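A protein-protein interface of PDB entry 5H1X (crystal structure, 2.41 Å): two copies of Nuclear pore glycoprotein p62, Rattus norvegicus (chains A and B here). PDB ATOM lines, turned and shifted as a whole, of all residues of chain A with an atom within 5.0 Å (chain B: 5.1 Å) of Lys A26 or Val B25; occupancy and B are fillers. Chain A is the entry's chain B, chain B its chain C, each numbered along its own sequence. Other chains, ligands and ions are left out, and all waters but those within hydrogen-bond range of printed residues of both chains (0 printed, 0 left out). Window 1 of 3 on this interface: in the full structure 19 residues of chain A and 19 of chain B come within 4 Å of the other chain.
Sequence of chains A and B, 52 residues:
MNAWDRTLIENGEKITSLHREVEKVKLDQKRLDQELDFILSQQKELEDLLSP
Among the printed residues, merely in contact across the chains: Lys A26 with Val B25, Gln A29 with Asp B28, Val A22 with Val B22, Val A25 with Val B25 and Val A22 with Glu B21.
OE1 of Glu A23 lies within salt-bridge range of NZ of Lys A26, at 2.7 Å.
OE2 of Glu B21 is in salt-bridge range of NZ of Lys B24 (3.6 Å).
Val A22 touches its own counterpart, Val B22.
Val A25 touches its own counterpart, Val B25.
Gln A29 touches Val B25, but with the chains exchanged Val A25 does not touch Gln B29 (4.7 Å).
Gln A29 touches Asp B28, but with the chains exchanged Asp A28 does not touch Gln B29 (8.5 Å).
Positions printed for both chains: 22, 23, 24, 25, 26, 27, 28, 29 and 30.
Of the 8 pairs that touch across the chains among the printed residues, 3 have their exchanged pair printed and touching as well.
Of the 9 printed residues of chain A, 4 touch a printed residue of chain B.
Along chain A the printed residues that touch a printed residue of chain B span positions 22 to 29.
Hydrophobic or aromatic side chains of chain B that line the printed part of chain A: Val B22 and Val B25.
Among the printed residues, Asp or Glu carboxylates within 4 Å of a Lys or Arg side-chain nitrogen of the other chain: Lys A26 with Glu B21.
Printed residues of chain B within 4 Å of Val A22: Glu B21 and Val B22.
Of chain B, only Glu B21 (3.0 Å) and Val B25 (3.5 Å) come within 4 Å of Lys A26.
Of the printed residues of chain B, Gln A29 touches Val B25 (3.1 Å), Asp B28 (3.5 Å) and Gln B29 (3.3 Å).
Lys A30 touches none of the printed residues of chain B.
Printed residues of chain A within 4 Å of Glu B21: Val A22 (3.9 Å) and Lys A26 (3.0 Å).
Leu B27 touches none of the printed residues of chain A.
Of the printed residues of chain A, Asp B28 touches Gln A29 (3.5 Å).
Printed residues of chain A within 4 Å of Gln B29: Gln A29 (3.3 Å).
The nearest printed residue of chain B that does not touch Lys A26 is Val B22 (6.7 Å).
The nearest printed residue of chain A that does not touch Val B25 is Val A22 (5.1 Å).
The nearest printed residue of chain A that does not touch Val B22 is Lys A26 (6.7 Å).
The side-chain carboxylate of Glu B21 is in salt-bridge range of the side-chain amino group of Lys A26 (3.0 Å).
O of Val B25 sits at hydrogen-bond distance from NE2 of Gln A29 (3.1 Å).
The backbone NH of Gln B29 sits close to the side-chain amide nitrogen of Gln A29 (3.3 Å).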
ATOM      1  N   VAL A  22      -1.680  14.493  28.412  1.00  0.00           N
ATOM      2  CA  VAL A  22      -2.754  14.889  27.512  1.00  0.00           C
ATOM      3  C   VAL A  22      -3.755  15.773  28.242  1.00  0.00           C
ATOM      4  O   VAL A  22      -4.183  16.805  27.711  1.00  0.00           O
ATOM      5  CB  VAL A  22      -3.444  13.681  26.896  1.00  0.00           C
ATOM      6  CG1 VAL A  22      -4.919  13.924  26.708  1.00  0.00           C
ATOM      7  CG2 VAL A  22      -2.805  13.378  25.570  1.00  0.00           C
ATOM      8  N   GLU A  23      -4.068  15.401  29.475  1.00  0.00           N
ATOM      9  CA  GLU A  23      -4.980  16.172  30.307  1.00  0.00           C
ATOM     10  C   GLU A  23      -4.479  17.610  30.476  1.00  0.00           C
ATOM     11  O   GLU A  23      -5.243  18.560  30.407  1.00  0.00           O
ATOM     12  CB  GLU A  23      -5.139  15.494  31.673  1.00  0.00           C
ATOM     13  CG  GLU A  23      -6.413  15.863  32.436  1.00  0.00           C
ATOM     14  CD  GLU A  23      -7.698  15.364  31.767  1.00  0.00           C
ATOM     15  OE1 GLU A  23      -7.628  14.558  30.810  1.00  0.00           O
ATOM     16  OE2 GLU A  23      -8.788  15.782  32.211  1.00  0.00           O
ATOM     17  N   LYS A  24      -3.178  17.746  30.689  1.00  0.00           N
ATOM     18  CA  LYS A  24      -2.554  19.031  30.897  1.00  0.00           C
ATOM     19  C   LYS A  24      -2.637  19.892  29.638  1.00  0.00           C
ATOM     20  O   LYS A  24      -2.900  21.090  29.721  1.00  0.00           O
ATOM     21  CB  LYS A  24      -1.109  18.816  31.332  1.00  0.00           C
ATOM     22  CG  LYS A  24      -0.105  19.859  30.897  1.00  0.00           C
ATOM     23  CD  LYS A  24       1.300  19.251  31.036  1.00  0.00           C
ATOM     24  CE  LYS A  24       1.476  18.533  32.390  1.00  0.00           C
ATOM     25  NZ  LYS A  24       2.704  17.671  32.473  1.00  0.00           N
ATOM     26  N   VAL A  25      -2.444  19.269  28.476  1.00  0.00           N
ATOM     27  CA  VAL A  25      -2.609  19.939  27.192  1.00  0.00           C
ATOM     28  C   VAL A  25      -4.059  20.364  26.963  1.00  0.00           C
ATOM     29  O   VAL A  25      -4.327  21.491  26.522  1.00  0.00           O
ATOM     30  CB  VAL A  25      -2.162  19.045  26.030  1.00  0.00           C
ATOM     31  CG1 VAL A  25      -2.791  19.503  24.729  1.00  0.00           C
ATOM     32  CG2 VAL A  25      -0.640  19.013  25.944  1.00  0.00           C
ATOM     33  N   LYS A  26      -4.992  19.478  27.293  1.00  0.00           N
ATOM     34  CA  LYS A  26      -6.411  19.812  27.174  1.00  0.00           C
ATOM     35  C   LYS A  26      -6.801  21.027  28.019  1.00  0.00           C
ATOM     36  O   LYS A  26      -7.743  21.750  27.685  1.00  0.00           O
ATOM     37  CB  LYS A  26      -7.280  18.619  27.569  1.00  0.00           C
ATOM     38  CG  LYS A  26      -7.488  17.612  26.453  1.00  0.00           C
ATOM     39  CD  LYS A  26      -7.850  16.226  27.013  1.00  0.00           C
ATOM     40  CE  LYS A  26      -9.078  16.282  27.920  1.00  0.00           C
ATOM     41  NZ  LYS A  26      -9.225  15.025  28.730  1.00  0.00           N
ATOM     42  N   LEU A  27      -6.074  21.246  29.111  1.00  0.00           N
ATOM     43  CA  LEU A  27      -6.392  22.347  30.010  1.00  0.00           C
ATOM     44  C   LEU A  27      -5.881  23.660  29.442  1.00  0.00           C
ATOM     45  O   LEU A  27      -6.567  24.674  29.507  1.00  0.00           O
ATOM     46  CB  LEU A  27      -5.806  22.099  31.396  1.00  0.00           C
ATOM     47  CG  LEU A  27      -6.808  22.371  32.512  1.00  0.00           C
ATOM     48  CD1 LEU A  27      -8.041  21.487  32.331  1.00  0.00           C
ATOM     49  CD2 LEU A  27      -6.171  22.150  33.870  1.00  0.00           C
ATOM     50  N   ASP A  28      -4.676  23.629  28.881  1.00  0.00           N
ATOM     51  CA  ASP A  28      -4.117  24.789  28.188  1.00  0.00           C
ATOM     52  C   ASP A  28      -4.977  25.174  26.988  1.00  0.00           C
ATOM     53  O   ASP A  28      -5.301  26.347  26.808  1.00  0.00           O
ATOM     54  CB  ASP A  28      -2.678  24.516  27.742  1.00  0.00           C
ATOM     55  CG  ASP A  28      -1.714  24.452  28.905  1.00  0.00           C
ATOM     56  OD1 ASP A  28      -1.913  25.200  29.884  1.00  0.00           O
ATOM     57  OD2 ASP A  28      -0.756  23.655  28.850  1.00  0.00           O
ATOM     58  N   GLN A  29      -5.349  24.186  26.173  1.00  0.00           N
ATOM     59  CA  GLN A  29      -6.264  24.431  25.054  1.00  0.00           C
ATOM     60  C   GLN A  29      -7.518  25.158  25.502  1.00  0.00           C
ATOM     61  O   GLN A  29      -7.937  26.129  24.883  1.00  0.00           O
ATOM     62  CB  GLN A  29      -6.678  23.129  24.368  1.00  0.00           C
ATOM     63  CG  GLN A  29      -5.609  22.496  23.523  1.00  0.00           C
ATOM     64  CD  GLN A  29      -6.182  21.426  22.635  1.00  0.00           C
ATOM     65  OE1 GLN A  29      -6.774  20.449  23.112  1.00  0.00           O
ATOM     66  NE2 GLN A  29      -6.042  21.609  21.330  1.00  0.00           N
ATOM     67  N   LYS A  30      -8.111  24.651  26.577  1.00  0.00           N
ATOM     68  CA  LYS A  30      -9.332  25.196  27.135  1.00  0.00           C
ATOM     69  C   LYS A  30      -9.122  26.653  27.554  1.00  0.00           C
ATOM     70  O   LYS A  30      -9.988  27.496  27.339  1.00  0.00           O
ATOM     71  CB  LYS A  30      -9.785  24.335  28.318  1.00  0.00           C
ATOM     72  CG  LYS A  30     -10.432  25.094  29.471  1.00  0.00           C
ATOM     73  CD  LYS A  30     -11.486  24.248  30.197  1.00  0.00           C
ATOM     74  CE  LYS A  30     -12.128  25.032  31.344  1.00  0.00           C
ATOM     75  NZ  LYS A  30     -13.555  25.375  31.069  1.00  0.00           N
ATOM     76  N   GLU B  21      -8.376  10.708  22.773  1.00  0.00           N
ATOM     77  CA  GLU B  21      -8.175  12.032  23.346  1.00  0.00           C
ATOM     78  C   GLU B  21      -7.174  12.812  22.492  1.00  0.00           C
ATOM     79  O   GLU B  21      -7.354  14.002  22.225  1.00  0.00           O
ATOM     80  CB  GLU B  21      -7.678  11.944  24.789  1.00  0.00           C
ATOM     81  CG  GLU B  21      -8.680  11.340  25.763  1.00  0.00           C
ATOM     82  CD  GLU B  21      -9.964  12.146  25.839  1.00  0.00           C
ATOM     83  OE1 GLU B  21     -10.058  13.024  26.724  1.00  0.00           O
ATOM     84  OE2 GLU B  21     -10.878  11.905  25.017  1.00  0.00           O
ATOM     85  N   VAL B  22      -6.136  12.116  22.042  1.00  0.00           N
ATOM     86  CA  VAL B  22      -5.090  12.743  21.274  1.00  0.00           C
ATOM     87  C   VAL B  22      -5.618  13.284  19.935  1.00  0.00           C
ATOM     88  O   VAL B  22      -5.278  14.395  19.550  1.00  0.00           O
ATOM     89  CB  VAL B  22      -3.929  11.767  21.052  1.00  0.00           C
ATOM     90  CG1 VAL B  22      -3.260  12.001  19.704  1.00  0.00           C
ATOM     91  CG2 VAL B  22      -2.929  11.916  22.179  1.00  0.00           C
ATOM     92  N   GLU B  23      -6.459  12.512  19.247  1.00  0.00           N
ATOM     93  CA  GLU B  23      -7.011  12.950  17.967  1.00  0.00           C
ATOM     94  C   GLU B  23      -7.952  14.143  18.131  1.00  0.00           C
ATOM     95  O   GLU B  23      -7.967  15.028  17.282  1.00  0.00           O
ATOM     96  CB  GLU B  23      -7.753  11.809  17.264  1.00  0.00           C
ATOM     97  CG  GLU B  23      -6.881  10.625  16.849  1.00  0.00           C
ATOM     98  CD  GLU B  23      -5.941  10.940  15.698  1.00  0.00           C
ATOM     99  OE1 GLU B  23      -6.360  11.632  14.741  1.00  0.00           O
ATOM    100  OE2 GLU B  23      -4.777  10.477  15.746  1.00  0.00           O
ATOM    101  N   LYS B  24      -8.732  14.166  19.210  1.00  0.00           N
ATOM    102  CA  LYS B  24      -9.654  15.276  19.454  1.00  0.00           C
ATOM    103  C   LYS B  24      -8.878  16.560  19.708  1.00  0.00           C
ATOM    104  O   LYS B  24      -9.298  17.657  19.316  1.00  0.00           O
ATOM    105  CB  LYS B  24     -10.588  14.973  20.635  1.00  0.00           C
ATOM    106  CG  LYS B  24     -11.628  13.887  20.325  1.00  0.00           C
ATOM    107  CD  LYS B  24     -12.272  13.287  21.582  1.00  0.00           C
ATOM    108  CE  LYS B  24     -13.092  14.298  22.363  1.00  0.00           C
ATOM    109  NZ  LYS B  24     -13.630  13.703  23.625  1.00  0.00           N
ATOM    110  N   VAL B  25      -7.731  16.411  20.360  1.00  0.00           N
ATOM    111  CA  VAL B  25      -6.908  17.547  20.699  1.00  0.00           C
ATOM    112  C   VAL B  25      -6.237  18.112  19.454  1.00  0.00           C
ATOM    113  O   VAL B  25      -6.220  19.325  19.259  1.00  0.00           O
ATOM    114  CB  VAL B  25      -5.881  17.172  21.748  1.00  0.00           C
ATOM    115  CG1 VAL B  25      -4.676  18.109  21.708  1.00  0.00           C
ATOM    116  CG2 VAL B  25      -6.535  17.217  23.103  1.00  0.00           C
ATOM    117  N   LYS B  26      -5.718  17.237  18.603  1.00  0.00           N
ATOM    118  CA  LYS B  26      -5.135  17.677  17.343  1.00  0.00           C
ATOM    119  C   LYS B  26      -6.141  18.474  16.522  1.00  0.00           C
ATOM    120  O   LYS B  26      -5.774  19.459  15.873  1.00  0.00           O
ATOM    121  CB  LYS B  26      -4.631  16.490  16.537  1.00  0.00           C
ATOM    122  CG  LYS B  26      -3.427  15.803  17.164  1.00  0.00           C
ATOM    123  CD  LYS B  26      -3.286  14.370  16.671  1.00  0.00           C
ATOM    124  CE  LYS B  26      -2.119  14.224  15.713  1.00  0.00           C
ATOM    125  NZ  LYS B  26      -1.842  12.802  15.356  1.00  0.00           N
ATOM    126  N   LEU B  27      -7.405  18.051  16.562  1.00  0.00           N
ATOM    127  CA  LEU B  27      -8.469  18.766  15.874  1.00  0.00           C
ATOM    128  C   LEU B  27      -8.602  20.204  16.406  1.00  0.00           C
ATOM    129  O   LEU B  27      -8.503  21.173  15.652  1.00  0.00           O
ATOM    130  CB  LEU B  27      -9.795  18.023  16.025  1.00  0.00           C
ATOM    131  CG  LEU B  27     -10.032  16.692  15.307  1.00  0.00           C
ATOM    132  CD1 LEU B  27     -11.389  16.138  15.705  1.00  0.00           C
ATOM    133  CD2 LEU B  27      -9.946  16.821  13.789  1.00  0.00           C
ATOM    134  N   ASP B  28      -8.811  20.334  17.710  1.00  0.00           N
ATOM    135  CA  ASP B  28      -8.899  21.643  18.340  1.00  0.00           C
ATOM    136  C   ASP B  28      -7.616  22.439  18.192  1.00  0.00           C
ATOM    137  O   ASP B  28      -7.663  23.667  18.166  1.00  0.00           O
ATOM    138  CB  ASP B  28      -9.250  21.519  19.820  1.00  0.00           C
ATOM    139  CG  ASP B  28     -10.730  21.299  20.048  1.00  0.00           C
ATOM    140  OD1 ASP B  28     -11.526  22.213  19.713  1.00  0.00           O
ATOM    141  OD2 ASP B  28     -11.091  20.220  20.579  1.00  0.00           O
ATOM    142  N   GLN B  29      -6.475  21.765  18.085  1.00  0.00           N
ATOM    143  CA  GLN B  29      -5.234  22.491  17.824  1.00  0.00           C
ATOM    144  C   GLN B  29      -5.316  23.191  16.478  1.00  0.00           C
ATOM    145  O   GLN B  29      -4.861  24.322  16.326  1.00  0.00           O
ATOM    146  CB  GLN B  29      -4.019  21.572  17.832  1.00  0.00           C
ATOM    147  CG  GLN B  29      -3.575  21.118  19.209  1.00  0.00           C
ATOM    148  CD  GLN B  29      -2.185  20.502  19.193  1.00  0.00           C
ATOM    149  OE1 GLN B  29      -1.697  20.045  18.145  1.00  0.00           O
ATOM    150  NE2 GLN B  29      -1.526  20.522  20.346  1.00  0.00           N
ATOM    151  N   LYS B  30      -5.889  22.500  15.499  1.00  0.00           N
ATOM    152  CA  LYS B  30      -6.022  23.057  14.169  1.00  0.00           C
ATOM    153  C   LYS B  30      -7.067  24.183  14.108  1.00  0.00           C
ATOM    154  O   LYS B  30      -6.912  25.126  13.335  1.00  0.00           O
ATOM    155  CB  LYS B  30      -6.368  21.954  13.177  1.00  0.00           C
ATOM    156  CG  LYS B  30      -5.492  21.968  11.930  1.00  0.00           C
ATOM    157  CD  LYS B  30      -4.004  22.106  12.275  1.00  0.00           C
ATOM    158  CE  LYS B  30      -3.123  21.723  11.085  1.00  0.00           C
ATOM    159  NZ  LYS B  30      -1.666  21.924  11.343  1.00  0.00           N
